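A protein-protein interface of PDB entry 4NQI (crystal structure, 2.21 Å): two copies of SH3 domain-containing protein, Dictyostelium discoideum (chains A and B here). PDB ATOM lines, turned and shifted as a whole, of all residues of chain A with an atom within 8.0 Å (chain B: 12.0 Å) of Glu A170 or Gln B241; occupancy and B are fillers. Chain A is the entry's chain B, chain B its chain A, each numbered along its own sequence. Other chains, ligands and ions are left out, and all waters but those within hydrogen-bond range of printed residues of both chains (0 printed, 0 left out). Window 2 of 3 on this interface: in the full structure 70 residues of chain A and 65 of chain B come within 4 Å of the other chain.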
ATOM      1  N   ASN A  14      26.166   9.181  36.444  1.00  0.00           N
ATOM      2  CA  ASN A  14      24.873   9.096  35.777  1.00  0.00           C
ATOM      3  C   ASN A  14      23.791   8.518  36.693  1.00  0.00           C
ATOM      4  O   ASN A  14      23.871   7.359  37.100  1.00  0.00           O
ATOM      5  CB  ASN A  14      24.989   8.265  34.497  1.00  0.00           C
ATOM      6  CG  ASN A  14      23.747   8.354  33.621  1.00  0.00           C
ATOM      7  OD1 ASN A  14      22.667   8.733  34.077  1.00  0.00           O
ATOM      8  ND2 ASN A  14      23.898   7.991  32.354  1.00  0.00           N
ATOM      9  N   PRO A  15      22.772   9.334  37.009  1.00  0.00           N
ATOM     10  CA  PRO A  15      21.626   8.984  37.861  1.00  0.00           C
ATOM     11  C   PRO A  15      20.794   7.802  37.349  1.00  0.00           C
ATOM     12  O   PRO A  15      20.450   6.932  38.151  1.00  0.00           O
ATOM     13  CB  PRO A  15      20.778  10.260  37.843  1.00  0.00           C
ATOM     14  CG  PRO A  15      21.745  11.350  37.555  1.00  0.00           C
ATOM     15  CD  PRO A  15      22.757  10.757  36.624  1.00  0.00           C
ATOM     16  N   VAL A  16      20.461   7.784  36.057  1.00  0.00           N
ATOM     17  CA  VAL A  16      19.693   6.684  35.462  1.00  0.00           C
ATOM     18  C   VAL A  16      20.366   5.332  35.706  1.00  0.00           C
ATOM     19  O   VAL A  16      19.733   4.382  36.175  1.00  0.00           O
ATOM     20  CB  VAL A  16      19.486   6.888  33.942  1.00  0.00           C
ATOM     21  CG1 VAL A  16      19.054   5.588  33.272  1.00  0.00           C
ATOM     22  CG2 VAL A  16      18.470   7.991  33.675  1.00  0.00           C
ATOM     23  N   ILE A  17      21.656   5.264  35.390  1.00  0.00           N
ATOM     24  CA  ILE A  17      22.463   4.069  35.612  1.00  0.00           C
ATOM     25  C   ILE A  17      22.591   3.733  37.103  1.00  0.00           C
ATOM     26  O   ILE A  17      22.548   2.560  37.488  1.00  0.00           O
ATOM     27  CB  ILE A  17      23.866   4.230  34.983  1.00  0.00           C
ATOM     28  CG1 ILE A  17      23.742   4.516  33.483  1.00  0.00           C
ATOM     29  CG2 ILE A  17      24.716   2.995  35.218  1.00  0.00           C
ATOM     30  N   MET A 132      27.222  -1.963  23.440  1.00  0.00           N
ATOM     31  CA  MET A 132      27.098  -0.555  23.076  1.00  0.00           C
ATOM     32  C   MET A 132      28.433   0.175  23.178  1.00  0.00           C
ATOM     33  O   MET A 132      28.738   1.047  22.361  1.00  0.00           O
ATOM     34  CB  MET A 132      26.068   0.131  23.965  1.00  0.00           C
ATOM     35  CG  MET A 132      25.211   1.119  23.223  1.00  0.00           C
ATOM     36  SD  MET A 132      24.253   0.220  21.800  1.00  0.00           S
ATOM     37  CE  MET A 132      23.001   1.627  21.369  1.00  0.00           C
ATOM     38  N   ASN A 163      27.020  10.566  17.396  1.00  0.00           N
ATOM     39  CA  ASN A 163      25.985  11.108  18.267  1.00  0.00           C
ATOM     40  C   ASN A 163      24.694  10.286  18.251  1.00  0.00           C
ATOM     41  O   ASN A 163      24.013  10.180  19.271  1.00  0.00           O
ATOM     42  CB  ASN A 163      25.695  12.570  17.914  1.00  0.00           C
ATOM     43  CG  ASN A 163      26.785  13.514  18.393  1.00  0.00           C
ATOM     44  OD1 ASN A 163      27.560  13.184  19.291  1.00  0.00           O
ATOM     45  ND2 ASN A 163      26.841  14.703  17.798  1.00  0.00           N
ATOM     46  N   ASP A 164      24.362   9.709  17.096  1.00  0.00           N
ATOM     47  CA  ASP A 164      23.174   8.863  16.974  1.00  0.00           C
ATOM     48  C   ASP A 164      23.290   7.609  17.838  1.00  0.00           C
ATOM     49  O   ASP A 164      22.322   7.192  18.474  1.00  0.00           O
ATOM     50  CB  ASP A 164      22.925   8.459  15.515  1.00  0.00           C
ATOM     51  CG  ASP A 164      22.212   9.537  14.714  1.00  0.00           C
ATOM     52  OD1 ASP A 164      21.799  10.556  15.306  1.00  0.00           O
ATOM     53  OD2 ASP A 164      22.057   9.355  13.488  1.00  0.00           O
ATOM     54  N   LYS A 165      24.478   7.012  17.855  1.00  0.00           N
ATOM     55  CA  LYS A 165      24.721   5.805  18.641  1.00  0.00           C
ATOM     56  C   LYS A 165      24.719   6.101  20.146  1.00  0.00           C
ATOM     57  O   LYS A 165      24.432   5.223  20.962  1.00  0.00           O
ATOM     58  CB  LYS A 165      26.045   5.155  18.229  1.00  0.00           C
ATOM     59  CG  LYS A 165      26.125   3.673  18.553  1.00  0.00           C
ATOM     60  CD  LYS A 165      25.239   2.859  17.621  1.00  0.00           C
ATOM     61  N   ILE A 166      25.034   7.345  20.501  1.00  0.00           N
ATOM     62  CA  ILE A 166      25.057   7.785  21.894  1.00  0.00           C
ATOM     63  C   ILE A 166      23.633   8.049  22.392  1.00  0.00           C
ATOM     64  O   ILE A 166      23.294   7.755  23.541  1.00  0.00           O
ATOM     65  CB  ILE A 166      25.943   9.047  22.055  1.00  0.00           C
ATOM     66  CG1 ILE A 166      27.409   8.705  21.760  1.00  0.00           C
ATOM     67  CG2 ILE A 166      25.804   9.650  23.444  1.00  0.00           C
ATOM     68  CD1 ILE A 166      28.348   9.897  21.811  1.00  0.00           C
ATOM     69  N   LYS A 167      22.805   8.591  21.503  1.00  0.00           N
ATOM     70  CA  LYS A 167      21.382   8.800  21.752  1.00  0.00           C
ATOM     71  C   LYS A 167      20.648   7.456  21.743  1.00  0.00           C
ATOM     72  O   LYS A 167      19.509   7.344  22.203  1.00  0.00           O
ATOM     73  CB  LYS A 167      20.822   9.727  20.670  1.00  0.00           C
ATOM     74  CG  LYS A 167      19.355  10.094  20.793  1.00  0.00           C
ATOM     75  N   GLU A 168      21.323   6.436  21.223  1.00  0.00           N
ATOM     76  CA  GLU A 168      20.781   5.085  21.142  1.00  0.00           C
ATOM     77  C   GLU A 168      21.146   4.312  22.414  1.00  0.00           C
ATOM     78  O   GLU A 168      20.355   3.513  22.921  1.00  0.00           O
ATOM     79  CB  GLU A 168      21.350   4.398  19.899  1.00  0.00           C
ATOM     80  CG  GLU A 168      20.605   3.168  19.407  1.00  0.00           C
ATOM     81  CD  GLU A 168      21.392   2.421  18.338  1.00  0.00           C
ATOM     82  OE1 GLU A 168      21.923   3.081  17.416  1.00  0.00           O
ATOM     83  OE2 GLU A 168      21.497   1.180  18.427  1.00  0.00           O
ATOM     84  N   SER A 169      22.352   4.563  22.919  1.00  0.00           N
ATOM     85  CA  SER A 169      22.822   3.994  24.180  1.00  0.00           C
ATOM     86  C   SER A 169      22.080   4.600  25.361  1.00  0.00           C
ATOM     87  O   SER A 169      21.782   3.918  26.343  1.00  0.00           O
ATOM     88  CB  SER A 169      24.317   4.267  24.343  1.00  0.00           C
ATOM     89  OG  SER A 169      24.731   4.062  25.683  1.00  0.00           O
ATOM     90  N   GLU A 170      21.798   5.893  25.260  1.00  0.00           N
ATOM     91  CA  GLU A 170      21.100   6.617  26.311  1.00  0.00           C
ATOM     92  C   GLU A 170      19.677   6.106  26.454  1.00  0.00           C
ATOM     93  O   GLU A 170      19.116   6.093  27.550  1.00  0.00           O
ATOM     94  CB  GLU A 170      21.085   8.110  25.987  1.00  0.00           C
ATOM     95  CG  GLU A 170      21.409   9.015  27.163  1.00  0.00           C
ATOM     96  CD  GLU A 170      22.878   8.976  27.552  1.00  0.00           C
ATOM     97  OE1 GLU A 170      23.638   8.166  26.978  1.00  0.00           O
ATOM     98  OE2 GLU A 170      23.276   9.765  28.434  1.00  0.00           O
ATOM     99  N   GLN A 171      19.098   5.681  25.336  1.00  0.00           N
ATOM    100  CA  GLN A 171      17.735   5.174  25.336  1.00  0.00           C
ATOM    101  C   GLN A 171      17.679   3.748  25.863  1.00  0.00           C
ATOM    102  O   GLN A 171      16.621   3.272  26.277  1.00  0.00           O
ATOM    103  CB  GLN A 171      17.129   5.249  23.936  1.00  0.00           C
ATOM    104  CG  GLN A 171      15.966   6.213  23.845  1.00  0.00           C
ATOM    105  CD  GLN A 171      15.108   6.187  25.095  1.00  0.00           C
ATOM    106  OE1 GLN A 171      14.366   5.232  25.334  1.00  0.00           O
ATOM    107  NE2 GLN A 171      15.213   7.234  25.906  1.00  0.00           N
ATOM    108  N   LEU A 172      18.823   3.072  25.838  1.00  0.00           N
ATOM    109  CA  LEU A 172      18.938   1.740  26.416  1.00  0.00           C
ATOM    110  C   LEU A 172      18.977   1.825  27.937  1.00  0.00           C
ATOM    111  O   LEU A 172      18.316   1.041  28.621  1.00  0.00           O
ATOM    112  CB  LEU A 172      20.192   1.031  25.901  1.00  0.00           C
ATOM    113  CG  LEU A 172      20.530  -0.307  26.568  1.00  0.00           C
ATOM    114  CD1 LEU A 172      19.433  -1.329  26.315  1.00  0.00           C
ATOM    115  CD2 LEU A 172      21.879  -0.835  26.092  1.00  0.00           C
ATOM    116  N   ASN A 173      19.750   2.775  28.462  1.00  0.00           N
ATOM    117  CA  ASN A 173      19.842   2.978  29.906  1.00  0.00           C
ATOM    118  C   ASN A 173      18.482   3.280  30.537  1.00  0.00           C
ATOM    119  O   ASN A 173      18.143   2.741  31.588  1.00  0.00           O
ATOM    120  CB  ASN A 173      20.827   4.104  30.240  1.00  0.00           C
ATOM    121  CG  ASN A 173      22.242   3.804  29.781  1.00  0.00           C
ATOM    122  OD1 ASN A 173      22.603   2.650  29.542  1.00  0.00           O
ATOM    123  ND2 ASN A 173      23.056   4.849  29.663  1.00  0.00           N
ATOM    124  N   ALA A 174      17.712   4.146  29.883  1.00  0.00           N
ATOM    125  CA  ALA A 174      16.393   4.539  30.375  1.00  0.00           C
ATOM    126  C   ALA A 174      15.378   3.401  30.257  1.00  0.00           C
ATOM    127  O   ALA A 174      14.528   3.228  31.133  1.00  0.00           O
ATOM    128  CB  ALA A 174      15.901   5.773  29.638  1.00  0.00           C
ATOM    129  N   ASN A 175      15.459   2.638  29.168  1.00  0.00           N
ATOM    130  CA  ASN A 175      14.609   1.462  28.993  1.00  0.00           C
ATOM    131  C   ASN A 175      14.889   0.404  30.059  1.00  0.00           C
ATOM    132  O   ASN A 175      13.970  -0.213  30.595  1.00  0.00           O
ATOM    133  CB  ASN A 175      14.799   0.857  27.595  1.00  0.00           C
ATOM    134  CG  ASN A 175      14.039   1.611  26.518  1.00  0.00           C
ATOM    135  OD1 ASN A 175      13.010   2.234  26.786  1.00  0.00           O
ATOM    136  ND2 ASN A 175      14.536   1.544  25.287  1.00  0.00           N
ATOM    137  N   LYS A 176      16.169   0.202  30.356  1.00  0.00           N
ATOM    138  CA  LYS A 176      16.587  -0.768  31.362  1.00  0.00           C
ATOM    139  C   LYS A 176      16.221  -0.319  32.773  1.00  0.00           C
ATOM    140  O   LYS A 176      16.069  -1.149  33.670  1.00  0.00           O
ATOM    141  CB  LYS A 176      18.093  -1.013  31.276  1.00  0.00           C
ATOM    142  CG  LYS A 176      18.547  -1.751  30.024  1.00  0.00           C
ATOM    143  CD  LYS A 176      17.761  -3.039  29.830  1.00  0.00           C
ATOM    144  CE  LYS A 176      18.390  -3.914  28.762  1.00  0.00           C
ATOM    145  NZ  LYS A 176      19.813  -4.192  29.074  1.00  0.00           N
ATOM    146  N   LEU B 230       5.163   3.509  36.030  1.00  0.00           N
ATOM    147  CA  LEU B 230       6.417   4.094  36.484  1.00  0.00           C
ATOM    148  C   LEU B 230       6.141   5.413  37.200  1.00  0.00           C
ATOM    149  O   LEU B 230       5.441   6.277  36.669  1.00  0.00           O
ATOM    150  CB  LEU B 230       7.361   4.328  35.304  1.00  0.00           C
ATOM    151  CG  LEU B 230       8.810   4.671  35.662  1.00  0.00           C
ATOM    152  CD1 LEU B 230       9.497   3.471  36.288  1.00  0.00           C
ATOM    153  CD2 LEU B 230       9.604   5.174  34.461  1.00  0.00           C
ATOM    154  N   LEU B 232       6.346   9.164  38.663  1.00  0.00           N
ATOM    155  CA  LEU B 232       6.721  10.426  38.022  1.00  0.00           C
ATOM    156  C   LEU B 232       8.169  10.809  38.307  1.00  0.00           C
ATOM    157  O   LEU B 232       8.852  11.362  37.444  1.00  0.00           O
ATOM    158  CB  LEU B 232       5.788  11.555  38.475  1.00  0.00           C
ATOM    159  CG  LEU B 232       4.621  11.952  37.568  1.00  0.00           C
ATOM    160  CD1 LEU B 232       3.942  10.727  36.989  1.00  0.00           C
ATOM    161  CD2 LEU B 232       3.611  12.801  38.332  1.00  0.00           C
ATOM    162  N   GLU B 233       8.633  10.511  39.518  1.00  0.00           N
ATOM    163  CA  GLU B 233      10.003  10.824  39.915  1.00  0.00           C
ATOM    164  C   GLU B 233      11.031  10.107  39.038  1.00  0.00           C
ATOM    165  O   GLU B 233      12.144  10.602  38.840  1.00  0.00           O
ATOM    166  CB  GLU B 233      10.228  10.472  41.387  1.00  0.00           C
ATOM    167  CG  GLU B 233      10.509  11.673  42.277  1.00  0.00           C
ATOM    168  CD  GLU B 233      11.137  11.281  43.600  1.00  0.00           C
ATOM    169  OE1 GLU B 233      10.396  11.134  44.594  1.00  0.00           O
ATOM    170  OE2 GLU B 233      12.376  11.121  43.643  1.00  0.00           O
ATOM    171  N   MET B 234      10.651   8.944  38.519  1.00  0.00           N
ATOM    172  CA  MET B 234      11.498   8.191  37.602  1.00  0.00           C
ATOM    173  C   MET B 234      11.434   8.805  36.206  1.00  0.00           C
ATOM    174  O   MET B 234      12.466   9.040  35.573  1.00  0.00           O
ATOM    175  CB  MET B 234      11.055   6.729  37.553  1.00  0.00           C
ATOM    176  CG  MET B 234      11.159   5.978  38.875  1.00  0.00           C
ATOM    177  SD  MET B 234      12.927   5.245  39.259  1.00  0.00           S
ATOM    178  CE  MET B 234      13.793   6.818  40.014  1.00  0.00           C
ATOM    179  N   GLU B 235      10.215   9.063  35.739  1.00  0.00           N
ATOM    180  CA  GLU B 235       9.979   9.661  34.424  1.00  0.00           C
ATOM    181  C   GLU B 235      10.658  11.023  34.269  1.00  0.00           C
ATOM    182  O   GLU B 235      11.161  11.360  33.196  1.00  0.00           O
ATOM    183  CB  GLU B 235       8.472   9.794  34.174  1.00  0.00           C
ATOM    184  CG  GLU B 235       7.728   8.462  34.048  1.00  0.00           C
ATOM    185  CD  GLU B 235       7.996   7.760  32.726  1.00  0.00           C
ATOM    186  OE1 GLU B 235       8.738   8.319  31.889  1.00  0.00           O
ATOM    187  OE2 GLU B 235       7.462   6.648  32.521  1.00  0.00           O
ATOM    188  N   SER B 236      10.671  11.796  35.352  1.00  0.00           N
ATOM    189  CA  SER B 236      11.290  13.117  35.370  1.00  0.00           C
ATOM    190  C   SER B 236      12.814  13.032  35.450  1.00  0.00           C
ATOM    191  O   SER B 236      13.521  13.879  34.899  1.00  0.00           O
ATOM    192  CB  SER B 236      10.740  13.937  36.539  1.00  0.00           C
ATOM    193  OG  SER B 236      11.789  14.474  37.323  1.00  0.00           O
ATOM    194  N   MET B 237      13.317  12.011  36.140  1.00  0.00           N
ATOM    195  CA  MET B 237      14.758  11.771  36.217  1.00  0.00           C
ATOM    196  C   MET B 237      15.327  11.388  34.850  1.00  0.00           C
ATOM    197  O   MET B 237      16.405  11.850  34.462  1.00  0.00           O
ATOM    198  CB  MET B 237      15.070  10.681  37.247  1.00  0.00           C
ATOM    199  CG  MET B 237      16.476  10.107  37.134  1.00  0.00           C
ATOM    200  SD  MET B 237      16.787   8.528  38.239  1.00  0.00           S
ATOM    201  CE  MET B 237      16.975   9.393  39.974  1.00  0.00           C
ATOM    202  N   ILE B 238      14.599  10.543  34.125  1.00  0.00           N
ATOM    203  CA  ILE B 238      14.980  10.157  32.770  1.00  0.00           C
ATOM    204  C   ILE B 238      15.083  11.387  31.867  1.00  0.00           C
ATOM    205  O   ILE B 238      16.085  11.579  31.176  1.00  0.00           O
ATOM    206  CB  ILE B 238      13.969   9.157  32.157  1.00  0.00           C
ATOM    207  CG1 ILE B 238      14.046   7.799  32.865  1.00  0.00           C
ATOM    208  CG2 ILE B 238      14.220   8.984  30.670  1.00  0.00           C
ATOM    209  CD1 ILE B 238      13.196   6.718  32.220  1.00  0.00           C
ATOM    210  N   SER B 239      14.042  12.218  31.885  1.00  0.00           N
ATOM    211  CA  SER B 239      13.995  13.429  31.070  1.00  0.00           C
ATOM    212  C   SER B 239      15.106  14.416  31.420  1.00  0.00           C
ATOM    213  O   SER B 239      15.614  15.118  30.547  1.00  0.00           O
ATOM    214  CB  SER B 239      12.632  14.112  31.199  1.00  0.00           C
ATOM    215  OG  SER B 239      11.624  13.384  30.521  1.00  0.00           O
ATOM    216  N   LYS B 240      15.480  14.466  32.695  1.00  0.00           N
ATOM    217  CA  LYS B 240      16.534  15.370  33.145  1.00  0.00           C
ATOM    218  C   LYS B 240      17.908  14.948  32.617  1.00  0.00           C
ATOM    219  O   LYS B 240      18.814  15.769  32.493  1.00  0.00           O
ATOM    220  CB  LYS B 240      16.548  15.445  34.675  1.00  0.00           C
ATOM    221  CG  LYS B 240      17.457  16.525  35.243  1.00  0.00           C
ATOM    222  N   GLN B 241      18.053  13.664  32.300  1.00  0.00           N
ATOM    223  CA  GLN B 241      19.319  13.138  31.799  1.00  0.00           C
ATOM    224  C   GLN B 241      19.531  13.491  30.327  1.00  0.00           C
ATOM    225  O   GLN B 241      20.670  13.587  29.861  1.00  0.00           O
ATOM    226  CB  GLN B 241      19.381  11.620  32.008  1.00  0.00           C
ATOM    227  CG  GLN B 241      20.718  10.974  31.646  1.00  0.00           C
ATOM    228  CD  GLN B 241      21.895  11.584  32.389  1.00  0.00           C
ATOM    229  OE1 GLN B 241      21.753  12.089  33.505  1.00  0.00           O
ATOM    230  NE2 GLN B 241      23.072  11.536  31.767  1.00  0.00           N
ATOM    231  N   GLU B 242      18.433  13.701  29.603  1.00  0.00           N
ATOM    232  CA  GLU B 242      18.505  14.066  28.192  1.00  0.00           C
ATOM    233  C   GLU B 242      18.981  15.506  28.000  1.00  0.00           C
ATOM    234  O   GLU B 242      19.358  15.901  26.896  1.00  0.00           O
ATOM    235  CB  GLU B 242      17.148  13.863  27.504  1.00  0.00           C
ATOM    236  CG  GLU B 242      16.623  12.431  27.552  1.00  0.00           C
ATOM    237  N   ARG B 243      18.959  16.287  29.078  1.00  0.00           N
ATOM    238  CA  ARG B 243      19.392  17.678  29.017  1.00  0.00           C
ATOM    239  C   ARG B 243      20.733  17.876  29.717  1.00  0.00           C
ATOM    240  O   ARG B 243      21.649  18.485  29.162  1.00  0.00           O
ATOM    241  CB  ARG B 243      18.335  18.602  29.625  1.00  0.00           C
ATOM    242  CG  ARG B 243      18.207  18.515  31.136  1.00  0.00           C
ATOM    243  CD  ARG B 243      17.156  19.488  31.634  1.00  0.00           C
ATOM    244  NE  ARG B 243      16.965  19.418  33.079  1.00  0.00           N
ATOM    245  CZ  ARG B 243      17.680  20.109  33.962  1.00  0.00           C
ATOM    246  NH1 ARG B 243      18.645  20.919  33.549  1.00  0.00           N
ATOM    247  NH2 ARG B 243      17.432  19.987  35.258  1.00  0.00           N
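The side-chain amide oxygen (OD1) of Asn A14 lies within hydrogen-bond range of the backbone NH (N) of Val A16, 3.1 Å away.
Among the printed residues, pairs that only touch across the chains: Asn A14 with Gln B241, Pro A15 with Met B237, Pro A15 with Gln B241, Glu A170 with Gln B241 and Ala A174 with Ile B238.
Of chain B, only Gln B241 comes within 4 Å of Glu A170.
Gln B241 touches just these residues of chain A: Asn A14, Pro A15 and Glu A170.
Of chain B, only Gln B241 (3.4 Å) comes within 4 Å of Asn A14.
No residue of chain B comes within 4 Å of Ile A166.
No residue of chain B comes within 4 Å of Ser A169.
No residue of chain B comes within 4 Å of Gln A171.
No residue of chain B comes within 4 Å of Asn A173.
Ala A174 touches just one residue of chain B: Ile B238 (3.8 Å).
Of the printed residues of chain B, Pro A15 touches Met B237 and Gln B241.
Printed residues of chain A within 4 Å of Met B237: Pro A15.
Of the printed residues of chain A, Ile B238 touches Ala A174 (3.8 Å).
Ile A17 touches none of the printed residues of chain B.
Arg B243 touches none of the printed residues of chain A.
The nearest residue of chain B that does not touch Glu A170 is Glu B242 (5.9 Å).
The nearest residue of chain A that does not touch Gln B241 is Val A16 (4.1 Å).
The nearest printed residue of chain A that does not touch Met B237 is Val A16 (4.3 Å).
Printed residues of chain A that touch a printed residue of chain B: Asn A14, Pro A15, Glu A170 and Ala A174.
Hydrophobic or aromatic side chains of chain A within 4 Å of the printed part of chain B: Pro A15 and Ala A174.
Hydrophobic or aromatic side chains of chain B that line the printed part of chain A: Met B237 and Ile B238.
Among the printed residues, 5 pairs touch across the chains.
Among the printed residues, no Asp or Glu carboxylate lies within 4 Å of a Lys or Arg side-chain nitrogen of the other chain.
No position is printed for both chains.
Of the 5 pairs that touch across the chains among the printed residues, none has its exchanged pair printed and touching as well.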
